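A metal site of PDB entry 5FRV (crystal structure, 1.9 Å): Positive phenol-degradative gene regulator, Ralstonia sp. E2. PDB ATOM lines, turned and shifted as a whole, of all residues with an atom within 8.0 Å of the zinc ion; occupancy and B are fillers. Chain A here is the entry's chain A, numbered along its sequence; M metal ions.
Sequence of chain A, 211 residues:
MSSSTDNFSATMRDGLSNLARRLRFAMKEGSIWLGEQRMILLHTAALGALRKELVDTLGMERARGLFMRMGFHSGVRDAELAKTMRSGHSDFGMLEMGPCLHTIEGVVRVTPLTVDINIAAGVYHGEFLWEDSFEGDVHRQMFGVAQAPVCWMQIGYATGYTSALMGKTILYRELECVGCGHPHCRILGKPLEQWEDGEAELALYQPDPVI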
ATOM      1  N   VAL A 108       7.248   5.772  17.277  1.00  0.00           N
ATOM      2  CA  VAL A 108       6.834   6.290  18.583  1.00  0.00           C
ATOM      3  C   VAL A 108       5.927   5.249  19.230  1.00  0.00           C
ATOM      4  O   VAL A 108       5.321   4.423  18.547  1.00  0.00           O
ATOM      5  CB  VAL A 108       6.105   7.680  18.466  1.00  0.00           C
ATOM      6  CG1 VAL A 108       4.848   7.588  17.587  1.00  0.00           C
ATOM      7  CG2 VAL A 108       5.721   8.249  19.853  1.00  0.00           C
ATOM      8  N   TRP A 130       2.431  10.262  23.369  1.00  0.00           N
ATOM      9  CA  TRP A 130       3.575   9.788  22.587  1.00  0.00           C
ATOM     10  C   TRP A 130       4.799   9.538  23.470  1.00  0.00           C
ATOM     11  O   TRP A 130       5.417  10.496  23.942  1.00  0.00           O
ATOM     12  CB  TRP A 130       3.936  10.815  21.514  1.00  0.00           C
ATOM     13  CG  TRP A 130       3.164  10.726  20.222  1.00  0.00           C
ATOM     14  CD1 TRP A 130       2.307   9.733  19.847  1.00  0.00           C
ATOM     15  CD2 TRP A 130       3.185  11.670  19.150  1.00  0.00           C
ATOM     16  NE1 TRP A 130       1.795  10.011  18.590  1.00  0.00           N
ATOM     17  CE2 TRP A 130       2.323  11.193  18.143  1.00  0.00           C
ATOM     18  CE3 TRP A 130       3.871  12.872  18.921  1.00  0.00           C
ATOM     19  CZ2 TRP A 130       2.129  11.872  16.945  1.00  0.00           C
ATOM     20  CZ3 TRP A 130       3.643  13.562  17.734  1.00  0.00           C
ATOM     21  CH2 TRP A 130       2.789  13.050  16.763  1.00  0.00           C
ATOM     22  N   SER A 133       9.278   9.138  21.173  1.00  0.00           N
ATOM     23  CA  SER A 133       9.259   9.699  19.831  1.00  0.00           C
ATOM     24  C   SER A 133      10.667   9.686  19.241  1.00  0.00           C
ATOM     25  O   SER A 133      11.571  10.318  19.802  1.00  0.00           O
ATOM     26  CB  SER A 133       8.707  11.122  19.833  1.00  0.00           C
ATOM     27  OG  SER A 133       7.403  11.177  20.392  1.00  0.00           O
ATOM     28  N   PHE A 134      10.878   8.981  18.133  1.00  0.00           N
ATOM     29  CA  PHE A 134      12.195   9.002  17.517  1.00  0.00           C
ATOM     30  C   PHE A 134      12.520  10.413  17.092  1.00  0.00           C
ATOM     31  O   PHE A 134      13.660  10.855  17.171  1.00  0.00           O
ATOM     32  CB  PHE A 134      12.276   8.052  16.311  1.00  0.00           C
ATOM     33  CG  PHE A 134      11.990   8.713  14.988  1.00  0.00           C
ATOM     34  CD1 PHE A 134      10.693   8.805  14.512  1.00  0.00           C
ATOM     35  CD2 PHE A 134      13.018   9.254  14.221  1.00  0.00           C
ATOM     36  CE1 PHE A 134      10.427   9.413  13.297  1.00  0.00           C
ATOM     37  CE2 PHE A 134      12.770   9.875  13.026  1.00  0.00           C
ATOM     38  CZ  PHE A 134      11.474   9.948  12.562  1.00  0.00           C
ATOM     39  N   GLU A 135      11.505  11.147  16.650  1.00  0.00           N
ATOM     40  CA  GLU A 135      11.744  12.384  15.925  1.00  0.00           C
ATOM     41  C   GLU A 135      12.218  13.474  16.883  1.00  0.00           C
ATOM     42  O   GLU A 135      13.152  14.244  16.577  1.00  0.00           O
ATOM     43  CB  GLU A 135      10.481  12.816  15.207  1.00  0.00           C
ATOM     44  CG  GLU A 135      10.758  13.804  14.118  1.00  0.00           C
ATOM     45  CD  GLU A 135       9.540  14.086  13.276  1.00  0.00           C
ATOM     46  OE1 GLU A 135       8.460  13.579  13.655  1.00  0.00           O
ATOM     47  OE2 GLU A 135       9.660  14.805  12.255  1.00  0.00           O
ATOM     48  N   GLY A 136      11.570  13.536  18.037  1.00  0.00           N
ATOM     49  CA  GLY A 136      11.959  14.485  19.068  1.00  0.00           C
ATOM     50  C   GLY A 136      13.360  14.172  19.582  1.00  0.00           C
ATOM     51  O   GLY A 136      14.159  15.075  19.799  1.00  0.00           O
ATOM     52  N   ASP A 137      13.646  12.873  19.763  1.00  0.00           N
ATOM     53  CA  ASP A 137      14.984  12.434  20.165  1.00  0.00           C
ATOM     54  C   ASP A 137      16.049  12.826  19.176  1.00  0.00           C
ATOM     55  O   ASP A 137      17.047  13.403  19.561  1.00  0.00           O
ATOM     56  CB  ASP A 137      15.024  10.909  20.359  1.00  0.00           C
ATOM     57  CG  ASP A 137      14.140  10.426  21.497  1.00  0.00           C
ATOM     58  OD1 ASP A 137      13.207  11.146  21.938  1.00  0.00           O
ATOM     59  OD2 ASP A 137      14.412   9.283  21.961  1.00  0.00           O
ATOM     60  N   ALA A 148       9.849  25.313  19.854  1.00  0.00           N
ATOM     61  CA  ALA A 148       8.505  24.828  19.514  1.00  0.00           C
ATOM     62  C   ALA A 148       8.536  23.328  19.201  1.00  0.00           C
ATOM     63  O   ALA A 148       9.605  22.786  18.878  1.00  0.00           O
ATOM     64  CB  ALA A 148       7.946  25.606  18.330  1.00  0.00           C
ATOM     65  N   PRO A 149       7.366  22.643  19.316  1.00  0.00           N
ATOM     66  CA  PRO A 149       7.329  21.203  19.025  1.00  0.00           C
ATOM     67  C   PRO A 149       7.998  20.829  17.701  1.00  0.00           C
ATOM     68  O   PRO A 149       7.991  21.613  16.746  1.00  0.00           O
ATOM     69  CB  PRO A 149       5.844  20.891  18.992  1.00  0.00           C
ATOM     70  CG  PRO A 149       5.272  21.839  19.990  1.00  0.00           C
ATOM     71  CD  PRO A 149       6.073  23.127  19.825  1.00  0.00           C
ATOM     72  N   VAL A 150       8.601  19.639  17.671  1.00  0.00           N
ATOM     73  CA  VAL A 150       9.490  19.228  16.589  1.00  0.00           C
ATOM     74  C   VAL A 150       9.147  17.889  15.928  1.00  0.00           C
ATOM     75  O   VAL A 150       9.781  17.523  14.962  1.00  0.00           O
ATOM     76  CB  VAL A 150      10.966  19.130  17.089  1.00  0.00           C
ATOM     77  CG1 VAL A 150      11.413  20.416  17.755  1.00  0.00           C
ATOM     78  CG2 VAL A 150      11.112  17.972  18.040  1.00  0.00           C
ATOM     79  N   CYS A 151       8.163  17.141  16.438  1.00  0.00           N
ATOM     80  CA  CYS A 151       7.785  15.861  15.830  1.00  0.00           C
ATOM     81  C   CYS A 151       6.898  16.048  14.571  1.00  0.00           C
ATOM     82  O   CYS A 151       5.728  15.668  14.532  1.00  0.00           O
ATOM     83  CB  CYS A 151       7.094  14.973  16.887  1.00  0.00           C
ATOM     84  SG  CYS A 151       8.217  14.540  18.317  1.00  0.00           S
ATOM     85  N   TRP A 152       7.505  16.630  13.534  1.00  0.00           N
ATOM     86  CA  TRP A 152       6.852  17.020  12.300  1.00  0.00           C
ATOM     87  C   TRP A 152       6.297  15.866  11.473  1.00  0.00           C
ATOM     88  O   TRP A 152       5.111  15.880  11.078  1.00  0.00           O
ATOM     89  CB  TRP A 152       7.841  17.798  11.426  1.00  0.00           C
ATOM     90  CG  TRP A 152       8.425  18.975  12.137  1.00  0.00           C
ATOM     91  CD1 TRP A 152       7.860  19.714  13.147  1.00  0.00           C
ATOM     92  CD2 TRP A 152       9.716  19.545  11.902  1.00  0.00           C
ATOM     93  NE1 TRP A 152       8.719  20.707  13.546  1.00  0.00           N
ATOM     94  CE2 TRP A 152       9.862  20.629  12.804  1.00  0.00           C
ATOM     95  CE3 TRP A 152      10.762  19.249  11.028  1.00  0.00           C
ATOM     96  CZ2 TRP A 152      11.017  21.394  12.852  1.00  0.00           C
ATOM     97  CZ3 TRP A 152      11.909  20.017  11.072  1.00  0.00           C
ATOM     98  CH2 TRP A 152      12.030  21.084  11.968  1.00  0.00           C
ATOM     99  N   GLN A 154       5.829  12.887  12.562  1.00  0.00           N
ATOM    100  CA  GLN A 154       4.921  12.129  13.390  1.00  0.00           C
ATOM    101  C   GLN A 154       3.530  12.778  13.361  1.00  0.00           C
ATOM    102  O   GLN A 154       2.508  12.092  13.265  1.00  0.00           O
ATOM    103  CB  GLN A 154       5.468  11.999  14.824  1.00  0.00           C
ATOM    104  CG  GLN A 154       6.791  11.235  14.877  1.00  0.00           C
ATOM    105  CD  GLN A 154       7.332  11.023  16.289  1.00  0.00           C
ATOM    106  OE1 GLN A 154       8.486  10.610  16.462  1.00  0.00           O
ATOM    107  NE2 GLN A 154       6.484  11.261  17.296  1.00  0.00           N
ATOM    108  N   ILE A 155       3.503  14.112  13.408  1.00  0.00           N
ATOM    109  CA  ILE A 155       2.240  14.870  13.310  1.00  0.00           C
ATOM    110  C   ILE A 155       1.616  14.738  11.917  1.00  0.00           C
ATOM    111  O   ILE A 155       0.406  14.582  11.791  1.00  0.00           O
ATOM    112  CB  ILE A 155       2.454  16.353  13.643  1.00  0.00           C
ATOM    113  CG1 ILE A 155       2.589  16.530  15.155  1.00  0.00           C
ATOM    114  CG2 ILE A 155       1.284  17.202  13.148  1.00  0.00           C
ATOM    115  CD1 ILE A 155       1.292  16.244  15.904  1.00  0.00           C
ATOM    116  N   GLU A 174       0.958  19.211  18.491  1.00  0.00           N
ATOM    117  CA  GLU A 174       1.554  18.755  19.731  1.00  0.00           C
ATOM    118  C   GLU A 174       1.372  19.803  20.786  1.00  0.00           C
ATOM    119  O   GLU A 174       1.834  20.922  20.604  1.00  0.00           O
ATOM    120  CB  GLU A 174       3.046  18.495  19.561  1.00  0.00           C
ATOM    121  CG  GLU A 174       3.430  17.345  18.679  1.00  0.00           C
ATOM    122  CD  GLU A 174       4.927  17.127  18.734  1.00  0.00           C
ATOM    123  OE1 GLU A 174       5.639  17.835  17.995  1.00  0.00           O
ATOM    124  OE2 GLU A 174       5.395  16.288  19.522  1.00  0.00           O
ATOM    125  N   LEU A 175       0.742  19.445  21.894  1.00  0.00           N
ATOM    126  CA  LEU A 175       0.538  20.383  23.002  1.00  0.00           C
ATOM    127  C   LEU A 175       1.756  20.407  23.927  1.00  0.00           C
ATOM    128  O   LEU A 175       1.996  21.380  24.666  1.00  0.00           O
ATOM    129  CB  LEU A 175      -0.716  19.995  23.786  1.00  0.00           C
ATOM    130  CG  LEU A 175      -1.971  19.842  22.910  1.00  0.00           C
ATOM    131  CD1 LEU A 175      -3.186  19.619  23.790  1.00  0.00           C
ATOM    132  CD2 LEU A 175      -2.148  21.042  21.987  1.00  0.00           C
ATOM    133  N   GLU A 176       2.511  19.314  23.901  1.00  0.00           N
ATOM    134  CA  GLU A 176       3.803  19.248  24.586  1.00  0.00           C
ATOM    135  C   GLU A 176       4.667  18.254  23.839  1.00  0.00           C
ATOM    136  O   GLU A 176       4.149  17.474  23.024  1.00  0.00           O
ATOM    137  CB  GLU A 176       3.652  18.868  26.059  1.00  0.00           C
ATOM    138  CG  GLU A 176       3.330  17.408  26.348  1.00  0.00           C
ATOM    139  CD  GLU A 176       3.090  17.142  27.828  1.00  0.00           C
ATOM    140  OE1 GLU A 176       4.081  16.840  28.546  1.00  0.00           O
ATOM    141  OE2 GLU A 176       1.918  17.229  28.272  1.00  0.00           O
ATOM    142  N   CYS A 177       5.965  18.264  24.108  1.00  0.00           N
ATOM    143  CA  CYS A 177       6.887  17.463  23.311  1.00  0.00           C
ATOM    144  C   CYS A 177       8.273  17.343  23.940  1.00  0.00           C
ATOM    145  O   CYS A 177       8.788  18.306  24.509  1.00  0.00           O
ATOM    146  CB  CYS A 177       7.020  18.055  21.917  1.00  0.00           C
ATOM    147  SG  CYS A 177       8.326  17.275  20.952  1.00  0.00           S
ATOM    148  N   VAL A 178       8.880  16.160  23.787  1.00  0.00           N
ATOM    149  CA  VAL A 178      10.194  15.904  24.345  1.00  0.00           C
ATOM    150  C   VAL A 178      11.236  16.798  23.719  1.00  0.00           C
ATOM    151  O   VAL A 178      12.256  17.106  24.348  1.00  0.00           O
ATOM    152  CB  VAL A 178      10.638  14.436  24.148  1.00  0.00           C
ATOM    153  CG1 VAL A 178       9.815  13.524  25.005  1.00  0.00           C
ATOM    154  CG2 VAL A 178      10.544  14.025  22.682  1.00  0.00           C
ATOM    155  N   GLY A 179      10.984  17.232  22.495  1.00  0.00           N
ATOM    156  CA  GLY A 179      11.930  18.068  21.781  1.00  0.00           C
ATOM    157  C   GLY A 179      12.102  19.400  22.473  1.00  0.00           C
ATOM    158  O   GLY A 179      13.043  20.134  22.178  1.00  0.00           O
ATOM    159  N   CYS A 180      11.195  19.680  23.407  1.00  0.00           N
ATOM    160  CA  CYS A 180      11.188  20.934  24.151  1.00  0.00           C
ATOM    161  C   CYS A 180      11.527  20.721  25.622  1.00  0.00           C
ATOM    162  O   CYS A 180      11.371  21.629  26.435  1.00  0.00           O
ATOM    163  CB  CYS A 180       9.824  21.598  24.034  1.00  0.00           C
ATOM    164  SG  CYS A 180       9.344  21.903  22.337  1.00  0.00           S
ATOM    165  N   HIS A 182      10.172  18.330  27.588  1.00  0.00           N
ATOM    166  CA  HIS A 182       9.084  17.663  28.291  1.00  0.00           C
ATOM    167  C   HIS A 182       9.359  16.170  28.424  1.00  0.00           C
ATOM    168  O   HIS A 182      10.156  15.616  27.665  1.00  0.00           O
ATOM    169  CB  HIS A 182       7.758  17.885  27.561  1.00  0.00           C
ATOM    170  CG  HIS A 182       7.365  19.332  27.435  1.00  0.00           C
ATOM    171  ND1 HIS A 182       7.312  19.979  26.223  1.00  0.00           N
ATOM    172  CD2 HIS A 182       6.983  20.232  28.365  1.00  0.00           C
ATOM    173  CE1 HIS A 182       6.924  21.228  26.411  1.00  0.00           C
ATOM    174  NE2 HIS A 182       6.722  21.413  27.701  1.00  0.00           N
ATOM    175  N   HIS A 184       7.461  13.701  27.667  1.00  0.00           N
ATOM    176  CA  HIS A 184       6.863  12.965  26.572  1.00  0.00           C
ATOM    177  C   HIS A 184       6.214  13.951  25.623  1.00  0.00           C
ATOM    178  O   HIS A 184       6.249  15.157  25.868  1.00  0.00           O
ATOM    179  CB  HIS A 184       5.854  11.934  27.087  1.00  0.00           C
ATOM    180  CG  HIS A 184       4.904  12.472  28.114  1.00  0.00           C
ATOM    181  ND1 HIS A 184       4.020  13.498  27.836  1.00  0.00           N
ATOM    182  CD2 HIS A 184       4.703  12.137  29.406  1.00  0.00           C
ATOM    183  CE1 HIS A 184       3.310  13.767  28.920  1.00  0.00           C
ATOM    184  NE2 HIS A 184       3.707  12.961  29.889  1.00  0.00           N
ATOM    185  N   CYS A 185       5.647  13.444  24.522  1.00  0.00           N
ATOM    186  CA  CYS A 185       4.867  14.285  23.616  1.00  0.00           C
ATOM    187  C   CYS A 185       3.409  14.003  23.856  1.00  0.00           C
ATOM    188  O   CYS A 185       3.055  12.953  24.396  1.00  0.00           O
ATOM    189  CB  CYS A 185       5.232  14.041  22.142  1.00  0.00           C
ATOM    190  SG  CYS A 185       6.980  14.229  21.681  1.00  0.00           S
ATOM    191  N   ARG A 186       2.549  14.931  23.464  1.00  0.00           N
ATOM    192  CA  ARG A 186       1.106  14.776  23.628  1.00  0.00           C
ATOM    193  C   ARG A 186       0.400  15.620  22.590  1.00  0.00           C
ATOM    194  O   ARG A 186       0.734  16.790  22.377  1.00  0.00           O
ATOM    195  CB  ARG A 186       0.687  15.164  25.038  1.00  0.00           C
ATOM    196  CG  ARG A 186      -0.798  15.168  25.298  1.00  0.00           C
ATOM    197  CD  ARG A 186      -1.041  15.410  26.771  1.00  0.00           C
ATOM    198  NE  ARG A 186      -2.409  15.837  27.051  1.00  0.00           N
ATOM    199  CZ  ARG A 186      -2.823  17.092  26.992  1.00  0.00           C
ATOM    200  NH1 ARG A 186      -1.965  18.056  26.670  1.00  0.00           N
ATOM    201  NH2 ARG A 186      -4.093  17.403  27.267  1.00  0.00           N
ATOM    202  N   ILE A 187      -0.585  15.024  21.921  1.00  0.00           N
ATOM    203  CA  ILE A 187      -1.140  15.636  20.734  1.00  0.00           C
ATOM    204  C   ILE A 187      -2.673  15.730  20.785  1.00  0.00           C
ATOM    205  O   ILE A 187      -3.347  15.023  21.541  1.00  0.00           O
ATOM    206  CB  ILE A 187      -0.732  14.848  19.451  1.00  0.00           C
ATOM    207  CG1 ILE A 187      -1.564  13.574  19.303  1.00  0.00           C
ATOM    208  CG2 ILE A 187       0.783  14.539  19.471  1.00  0.00           C
ATOM    209  CD1 ILE A 187      -1.225  12.719  18.086  1.00  0.00           C
HETATM  210 ZN    ZN M   1       7.209  15.640  20.022  1.00  0.00          ZN
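OE2 of Glu 174 binds the zinc ion (2.0 Å). The zinc ion is bound by SG of Cys 177, 2.2 Å away. The side-chain sulfur (SG) of Cys 185 is bound to the zinc ion, 2.2 Å away. The zinc ion is bound by SG of Cys 151 (2.3 Å).
Four residues have an atom within 4 Å of the zinc ion: Cys 151, Glu 174, Cys 177 and Cys 185.
N of Val 150 sits at hydrogen-bond distance from OE1 of Glu 174 (3.5 Å). N of Gly 179 sits close to SG of Cys 177 (3.1 Å). ND1 of His 182 sits at hydrogen-bond distance from O of Cys 177, at 2.8 Å. The side-chain sulfur of Cys 185 sits close to the backbone NH of Val 178 (3.4 Å). The backbone carbonyl oxygen of Cys 185 lies within hydrogen-bond range of the backbone NH of Trp 130, at 2.9 Å. SG of Cys 185 lies close to OG of Ser 133. SG of Cys 151 sits close to N of Gly 136 (3.5 Å).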
